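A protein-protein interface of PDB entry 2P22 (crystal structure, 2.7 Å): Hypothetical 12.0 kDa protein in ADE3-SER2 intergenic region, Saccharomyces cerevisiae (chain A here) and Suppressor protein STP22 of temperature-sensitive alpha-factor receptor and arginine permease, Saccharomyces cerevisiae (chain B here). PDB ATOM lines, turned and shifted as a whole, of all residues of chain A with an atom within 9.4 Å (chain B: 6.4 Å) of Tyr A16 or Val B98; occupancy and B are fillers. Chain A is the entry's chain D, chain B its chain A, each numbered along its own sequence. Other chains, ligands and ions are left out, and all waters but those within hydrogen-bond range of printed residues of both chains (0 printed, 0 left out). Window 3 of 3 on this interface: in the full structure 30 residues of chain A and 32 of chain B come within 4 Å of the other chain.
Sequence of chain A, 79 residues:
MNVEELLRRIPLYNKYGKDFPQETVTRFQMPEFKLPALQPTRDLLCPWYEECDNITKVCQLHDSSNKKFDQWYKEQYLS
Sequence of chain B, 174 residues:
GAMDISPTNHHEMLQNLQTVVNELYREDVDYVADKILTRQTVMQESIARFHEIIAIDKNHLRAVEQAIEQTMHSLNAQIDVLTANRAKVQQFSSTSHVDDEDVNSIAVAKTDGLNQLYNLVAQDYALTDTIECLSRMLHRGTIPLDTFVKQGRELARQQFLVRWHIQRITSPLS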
ATOM      1  N   TYR A  13      30.295 -20.347   7.358  1.00  0.00           N
ATOM      2  CA  TYR A  13      28.942 -20.340   7.890  1.00  0.00           C
ATOM      3  C   TYR A  13      28.471 -18.932   8.230  1.00  0.00           C
ATOM      4  O   TYR A  13      29.267 -17.994   8.308  1.00  0.00           O
ATOM      5  CB  TYR A  13      28.836 -21.241   9.134  1.00  0.00           C
ATOM      6  CG  TYR A  13      28.752 -22.737   8.858  1.00  0.00           C
ATOM      7  CD1 TYR A  13      29.811 -23.427   8.249  1.00  0.00           C
ATOM      8  CD2 TYR A  13      27.624 -23.467   9.237  1.00  0.00           C
ATOM      9  CE1 TYR A  13      29.745 -24.817   8.025  1.00  0.00           C
ATOM     10  CE2 TYR A  13      27.541 -24.848   9.024  1.00  0.00           C
ATOM     11  CZ  TYR A  13      28.602 -25.521   8.418  1.00  0.00           C
ATOM     12  OH  TYR A  13      28.515 -26.885   8.203  1.00  0.00           O
ATOM     13  N   ASN A  14      27.160 -18.797   8.405  1.00  0.00           N
ATOM     14  CA  ASN A  14      26.556 -17.517   8.746  1.00  0.00           C
ATOM     15  C   ASN A  14      26.421 -17.421  10.254  1.00  0.00           C
ATOM     16  O   ASN A  14      25.642 -18.160  10.853  1.00  0.00           O
ATOM     17  CB  ASN A  14      25.162 -17.387   8.140  1.00  0.00           C
ATOM     18  CG  ASN A  14      24.569 -16.007   8.362  1.00  0.00           C
ATOM     19  OD1 ASN A  14      24.586 -15.164   7.469  1.00  0.00           O
ATOM     20  ND2 ASN A  14      24.068 -15.762   9.566  1.00  0.00           N
ATOM     21  N   LYS A  15      27.168 -16.508  10.863  1.00  0.00           N
ATOM     22  CA  LYS A  15      27.127 -16.331  12.307  1.00  0.00           C
ATOM     23  C   LYS A  15      25.791 -16.783  12.885  1.00  0.00           C
ATOM     24  O   LYS A  15      25.760 -17.663  13.739  1.00  0.00           O
ATOM     25  CB  LYS A  15      27.383 -14.870  12.656  1.00  0.00           C
ATOM     26  CG  LYS A  15      27.287 -14.557  14.124  1.00  0.00           C
ATOM     27  CD  LYS A  15      27.389 -13.054  14.347  1.00  0.00           C
ATOM     28  CE  LYS A  15      27.103 -12.688  15.797  1.00  0.00           C
ATOM     29  NZ  LYS A  15      27.088 -11.211  15.982  1.00  0.00           N
ATOM     30  N   TYR A  16      24.688 -16.206  12.407  1.00  0.00           N
ATOM     31  CA  TYR A  16      23.357 -16.573  12.908  1.00  0.00           C
ATOM     32  C   TYR A  16      22.809 -17.799  12.187  1.00  0.00           C
ATOM     33  O   TYR A  16      22.751 -17.832  10.964  1.00  0.00           O
ATOM     34  CB  TYR A  16      22.386 -15.401  12.744  1.00  0.00           C
ATOM     35  CG  TYR A  16      23.020 -14.060  13.039  1.00  0.00           C
ATOM     36  CD1 TYR A  16      23.818 -13.419  12.088  1.00  0.00           C
ATOM     37  CD2 TYR A  16      22.849 -13.439  14.278  1.00  0.00           C
ATOM     38  CE1 TYR A  16      24.427 -12.195  12.367  1.00  0.00           C
ATOM     39  CE2 TYR A  16      23.455 -12.217  14.565  1.00  0.00           C
ATOM     40  CZ  TYR A  16      24.241 -11.604  13.606  1.00  0.00           C
ATOM     41  OH  TYR A  16      24.844 -10.404  13.885  1.00  0.00           O
ATOM     42  N   GLY A  17      22.408 -18.810  12.946  1.00  0.00           N
ATOM     43  CA  GLY A  17      21.894 -20.018  12.325  1.00  0.00           C
ATOM     44  C   GLY A  17      20.570 -19.789  11.640  1.00  0.00           C
ATOM     45  O   GLY A  17      20.496 -19.128  10.613  1.00  0.00           O
ATOM     46  N   LYS A  18      19.516 -20.346  12.214  1.00  0.00           N
ATOM     47  CA  LYS A  18      18.190 -20.194  11.655  1.00  0.00           C
ATOM     48  C   LYS A  18      17.622 -18.807  11.937  1.00  0.00           C
ATOM     49  O   LYS A  18      16.538 -18.479  11.467  1.00  0.00           O
ATOM     50  CB  LYS A  18      17.267 -21.276  12.224  1.00  0.00           C
ATOM     51  CG  LYS A  18      17.391 -21.479  13.735  1.00  0.00           C
ATOM     52  CD  LYS A  18      16.502 -22.618  14.209  1.00  0.00           C
ATOM     53  CE  LYS A  18      16.807 -22.989  15.642  1.00  0.00           C
ATOM     54  NZ  LYS A  18      16.612 -21.855  16.572  1.00  0.00           N
ATOM     55  N   ASP A  19      18.354 -17.996  12.699  1.00  0.00           N
ATOM     56  CA  ASP A  19      17.902 -16.643  13.033  1.00  0.00           C
ATOM     57  C   ASP A  19      18.019 -15.673  11.864  1.00  0.00           C
ATOM     58  O   ASP A  19      17.386 -14.616  11.852  1.00  0.00           O
ATOM     59  CB  ASP A  19      18.689 -16.083  14.223  1.00  0.00           C
ATOM     60  CG  ASP A  19      17.979 -16.293  15.546  1.00  0.00           C
ATOM     61  OD1 ASP A  19      16.825 -15.831  15.687  1.00  0.00           O
ATOM     62  OD2 ASP A  19      18.580 -16.913  16.444  1.00  0.00           O
ATOM     63  N   PHE A  20      18.841 -16.034  10.886  1.00  0.00           N
ATOM     64  CA  PHE A  20      19.042 -15.196   9.717  1.00  0.00           C
ATOM     65  C   PHE A  20      17.873 -15.366   8.773  1.00  0.00           C
ATOM     66  O   PHE A  20      17.524 -16.488   8.406  1.00  0.00           O
ATOM     67  CB  PHE A  20      20.312 -15.599   8.989  1.00  0.00           C
ATOM     68  CG  PHE A  20      20.901 -14.503   8.177  1.00  0.00           C
ATOM     69  CD1 PHE A  20      21.405 -13.372   8.801  1.00  0.00           C
ATOM     70  CD2 PHE A  20      20.973 -14.600   6.794  1.00  0.00           C
ATOM     71  CE1 PHE A  20      21.979 -12.351   8.066  1.00  0.00           C
ATOM     72  CE2 PHE A  20      21.547 -13.582   6.046  1.00  0.00           C
ATOM     73  CZ  PHE A  20      22.052 -12.453   6.685  1.00  0.00           C
ATOM     74  N   PRO A  21      17.267 -14.250   8.349  1.00  0.00           N
ATOM     75  CA  PRO A  21      16.121 -14.250   7.438  1.00  0.00           C
ATOM     76  C   PRO A  21      16.433 -14.768   6.036  1.00  0.00           C
ATOM     77  O   PRO A  21      17.526 -14.549   5.506  1.00  0.00           O
ATOM     78  CB  PRO A  21      15.692 -12.788   7.441  1.00  0.00           C
ATOM     79  CG  PRO A  21      16.992 -12.071   7.598  1.00  0.00           C
ATOM     80  CD  PRO A  21      17.678 -12.872   8.670  1.00  0.00           C
ATOM     81  N   GLN A  22      15.453 -15.452   5.448  1.00  0.00           N
ATOM     82  CA  GLN A  22      15.574 -16.018   4.104  1.00  0.00           C
ATOM     83  C   GLN A  22      14.271 -15.827   3.318  1.00  0.00           C
ATOM     84  O   GLN A  22      13.187 -15.729   3.902  1.00  0.00           O
ATOM     85  CB  GLN A  22      15.892 -17.517   4.182  1.00  0.00           C
ATOM     86  CG  GLN A  22      17.015 -17.883   5.136  1.00  0.00           C
ATOM     87  CD  GLN A  22      18.352 -17.278   4.746  1.00  0.00           C
ATOM     88  OE1 GLN A  22      19.278 -17.236   5.556  1.00  0.00           O
ATOM     89  NE2 GLN A  22      18.462 -16.812   3.504  1.00  0.00           N
ATOM     90  N   PHE B  92      14.452  -8.665  12.886  1.00  0.00           N
ATOM     91  CA  PHE B  92      15.765  -9.246  13.100  1.00  0.00           C
ATOM     92  C   PHE B  92      16.808  -8.136  13.057  1.00  0.00           C
ATOM     93  O   PHE B  92      17.897  -8.284  13.594  1.00  0.00           O
ATOM     94  CB  PHE B  92      16.059 -10.261  12.002  1.00  0.00           C
ATOM     95  CG  PHE B  92      17.454 -10.807  12.037  1.00  0.00           C
ATOM     96  CD1 PHE B  92      17.819 -11.759  12.979  1.00  0.00           C
ATOM     97  CD2 PHE B  92      18.403 -10.377  11.118  1.00  0.00           C
ATOM     98  CE1 PHE B  92      19.111 -12.277  13.003  1.00  0.00           C
ATOM     99  CE2 PHE B  92      19.695 -10.890  11.137  1.00  0.00           C
ATOM    100  CZ  PHE B  92      20.049 -11.841  12.080  1.00  0.00           C
ATOM    101  N   SER B  93      16.467  -7.024  12.416  1.00  0.00           N
ATOM    102  CA  SER B  93      17.393  -5.905  12.296  1.00  0.00           C
ATOM    103  C   SER B  93      17.323  -4.911  13.450  1.00  0.00           C
ATOM    104  O   SER B  93      17.758  -3.766  13.317  1.00  0.00           O
ATOM    105  CB  SER B  93      17.151  -5.168  10.981  1.00  0.00           C
ATOM    106  OG  SER B  93      15.829  -4.670  10.911  1.00  0.00           O
ATOM    107  N   SER B  94      16.784  -5.342  14.584  1.00  0.00           N
ATOM    108  CA  SER B  94      16.683  -4.458  15.735  1.00  0.00           C
ATOM    109  C   SER B  94      17.202  -5.122  17.002  1.00  0.00           C
ATOM    110  O   SER B  94      18.305  -4.819  17.458  1.00  0.00           O
ATOM    111  CB  SER B  94      15.233  -4.018  15.935  1.00  0.00           C
ATOM    112  OG  SER B  94      14.386  -5.136  16.115  1.00  0.00           O
ATOM    113  N   SER B  96      18.666  -7.525  17.477  1.00  0.00           N
ATOM    114  CA  SER B  96      19.728  -8.437  17.087  1.00  0.00           C
ATOM    115  C   SER B  96      20.723  -7.690  16.209  1.00  0.00           C
ATOM    116  O   SER B  96      20.547  -7.600  14.996  1.00  0.00           O
ATOM    117  CB  SER B  96      19.146  -9.630  16.332  1.00  0.00           C
ATOM    118  OG  SER B  96      18.203 -10.317  17.136  1.00  0.00           O
ATOM    119  N   HIS B  97      21.764  -7.148  16.837  1.00  0.00           N
ATOM    120  CA  HIS B  97      22.788  -6.394  16.125  1.00  0.00           C
ATOM    121  C   HIS B  97      23.191  -7.107  14.850  1.00  0.00           C
ATOM    122  O   HIS B  97      23.952  -8.075  14.881  1.00  0.00           O
ATOM    123  CB  HIS B  97      24.011  -6.188  17.022  1.00  0.00           C
ATOM    124  CG  HIS B  97      23.698  -5.506  18.319  1.00  0.00           C
ATOM    125  ND1 HIS B  97      23.015  -4.311  18.386  1.00  0.00           N
ATOM    126  CD2 HIS B  97      23.960  -5.860  19.599  1.00  0.00           C
ATOM    127  CE1 HIS B  97      22.868  -3.959  19.651  1.00  0.00           C
ATOM    128  NE2 HIS B  97      23.432  -4.883  20.408  1.00  0.00           N
ATOM    129  N   VAL B  98      22.669  -6.619  13.728  1.00  0.00           N
ATOM    130  CA  VAL B  98      22.960  -7.207  12.430  1.00  0.00           C
ATOM    131  C   VAL B  98      24.300  -6.714  11.898  1.00  0.00           C
ATOM    132  O   VAL B  98      24.488  -6.546  10.694  1.00  0.00           O
ATOM    133  CB  VAL B  98      21.861  -6.888  11.417  1.00  0.00           C
ATOM    134  CG1 VAL B  98      22.032  -7.761  10.192  1.00  0.00           C
ATOM    135  CG2 VAL B  98      20.506  -7.123  12.040  1.00  0.00           C
ATOM    136  N   ASP B  99      25.214  -6.471  12.832  1.00  0.00           N
ATOM    137  CA  ASP B  99      26.581  -6.038  12.562  1.00  0.00           C
ATOM    138  C   ASP B  99      26.847  -4.838  11.664  1.00  0.00           C
ATOM    139  O   ASP B  99      26.014  -4.429  10.854  1.00  0.00           O
ATOM    140  CB  ASP B  99      27.396  -7.221  12.017  1.00  0.00           C
ATOM    141  CG  ASP B  99      27.481  -8.377  12.998  1.00  0.00           C
ATOM    142  OD1 ASP B  99      27.961  -8.168  14.133  1.00  0.00           O
ATOM    143  OD2 ASP B  99      27.069  -9.500  12.632  1.00  0.00           O
ATOM    144  N   ASP B 100      28.043  -4.282  11.838  1.00  0.00           N
ATOM    145  CA  ASP B 100      28.523  -3.160  11.045  1.00  0.00           C
ATOM    146  C   ASP B 100      28.585  -3.826   9.671  1.00  0.00           C
ATOM    147  O   ASP B 100      28.813  -5.032   9.589  1.00  0.00           O
ATOM    148  CB  ASP B 100      29.922  -2.758  11.533  1.00  0.00           C
ATOM    149  CG  ASP B 100      30.390  -1.430  10.969  1.00  0.00           C
ATOM    150  OD1 ASP B 100      30.571  -1.334   9.741  1.00  0.00           O
ATOM    151  OD2 ASP B 100      30.579  -0.478  11.757  1.00  0.00           O
ATOM    152  N   GLU B 101      28.365  -3.062   8.605  1.00  0.00           N
ATOM    153  CA  GLU B 101      28.367  -3.605   7.238  1.00  0.00           C
ATOM    154  C   GLU B 101      29.454  -4.620   6.861  1.00  0.00           C
ATOM    155  O   GLU B 101      29.371  -5.240   5.798  1.00  0.00           O
ATOM    156  CB  GLU B 101      28.371  -2.453   6.225  1.00  0.00           C
ATOM    157  CG  GLU B 101      26.983  -1.910   5.914  1.00  0.00           C
ATOM    158  CD  GLU B 101      26.213  -2.802   4.956  1.00  0.00           C
ATOM    159  OE1 GLU B 101      26.398  -4.036   5.021  1.00  0.00           O
ATOM    160  OE2 GLU B 101      25.418  -2.273   4.146  1.00  0.00           O
ATOM    161  N   SER B 105      32.049 -10.318  10.025  1.00  0.00           N
ATOM    162  CA  SER B 105      31.420 -10.752  11.264  1.00  0.00           C
ATOM    163  C   SER B 105      30.317 -11.770  11.020  1.00  0.00           C
ATOM    164  O   SER B 105      30.030 -12.603  11.877  1.00  0.00           O
ATOM    165  CB  SER B 105      30.827  -9.549  12.010  1.00  0.00           C
ATOM    166  OG  SER B 105      31.833  -8.638  12.432  1.00  0.00           O
ATOM    167  N   ILE B 106      29.703 -11.710   9.846  1.00  0.00           N
ATOM    168  CA  ILE B 106      28.604 -12.613   9.525  1.00  0.00           C
ATOM    169  C   ILE B 106      29.061 -13.963   9.022  1.00  0.00           C
ATOM    170  O   ILE B 106      28.635 -14.998   9.531  1.00  0.00           O
ATOM    171  CB  ILE B 106      27.690 -11.995   8.472  1.00  0.00           C
ATOM    172  CG1 ILE B 106      27.351 -10.560   8.885  1.00  0.00           C
ATOM    173  CG2 ILE B 106      26.408 -12.826   8.344  1.00  0.00           C
ATOM    174  CD1 ILE B 106      27.078  -9.650   7.737  1.00  0.00           C
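The backbone carbonyl oxygen (O) of Ile B106 is in hydrogen-bond range of the backbone NH (N) of Lys A15, 2.5 Å away.
The backbone carbonyl oxygen of His B97 is in hydrogen-bond range of the side-chain hydroxyl of Tyr A16 (2.7 Å).
OH of Tyr A16 sits at hydrogen-bond distance from OD2 of Asp B99, at 2.7 Å.
O of Ile B106 lies close to O of Tyr A13 (3.3 Å).
OD1 of Asp B99 lies within salt-bridge range of NZ of Lys A15 (3.7 Å).
The side-chain amino group (NZ) of Lys A15 is in hydrogen-bond range of the side-chain hydroxyl (OH) of Tyr A16 (3.2 Å).
The backbone carbonyl oxygen (O) of Tyr A16 sits at hydrogen-bond distance from the side-chain amide nitrogen (ND2) of Asn A14 (2.8 Å).
The backbone carbonyl oxygen (O) of Phe A20 lies close to the side-chain amide oxygen (OE1) of Gln A22 (3.4 Å).
Asn A14 touches Ile B106.
O of Ser B105 touches CB of Lys A15, 3.6 Å away.
Phe B92 touches Tyr A16.
CA of Val B98 touches OH of Tyr A16 (3.99 Å).
O of Asp A19 touches CD1 of Phe B92, 3.1 Å away.
Phe A20 touches Phe B92 (CD1 to CE2, 3.8 Å).
Pro A21 touches Phe B92.
Printed residues of chain B within 4 Å of Tyr A16: Phe B92 (3.8 Å), His B97 (2.7 Å), Val B98 (3.99 Å) and Asp B99 (2.7 Å).
Of the printed residues of chain A, Val B98 touches Tyr A16 (3.99 Å).
Asp B99 touches two residues of chain A.
Of the printed residues of chain B, Lys A15 touches Asp B99 (3.7 Å), Ser B105 (3.6 Å) and Ile B106 (2.5 Å).
Of the printed residues of chain B, Asn A14 touches Ile B106.
Ser B93 touches none of the printed residues of chain A.
Gln A22 touches none of the printed residues of chain B.
The nearest printed residue of chain A that does not touch Val B98 is Phe A20 (5.1 Å).
Printed residues of chain A that touch a printed residue of chain B: Tyr A13, Asn A14, Lys A15, Tyr A16, Asp A19, Phe A20 and Pro A21.
Hydrophobic or aromatic side chains of chain A within 4 Å of the printed part of chain B: Tyr A16, Phe A20 and Pro A21.
Along chain A the printed residues that touch a printed residue of chain B span positions 13 to 21.
Hydrophobic or aromatic side chains of chain B that line the printed part of chain A: Phe B92 and Ile B106.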
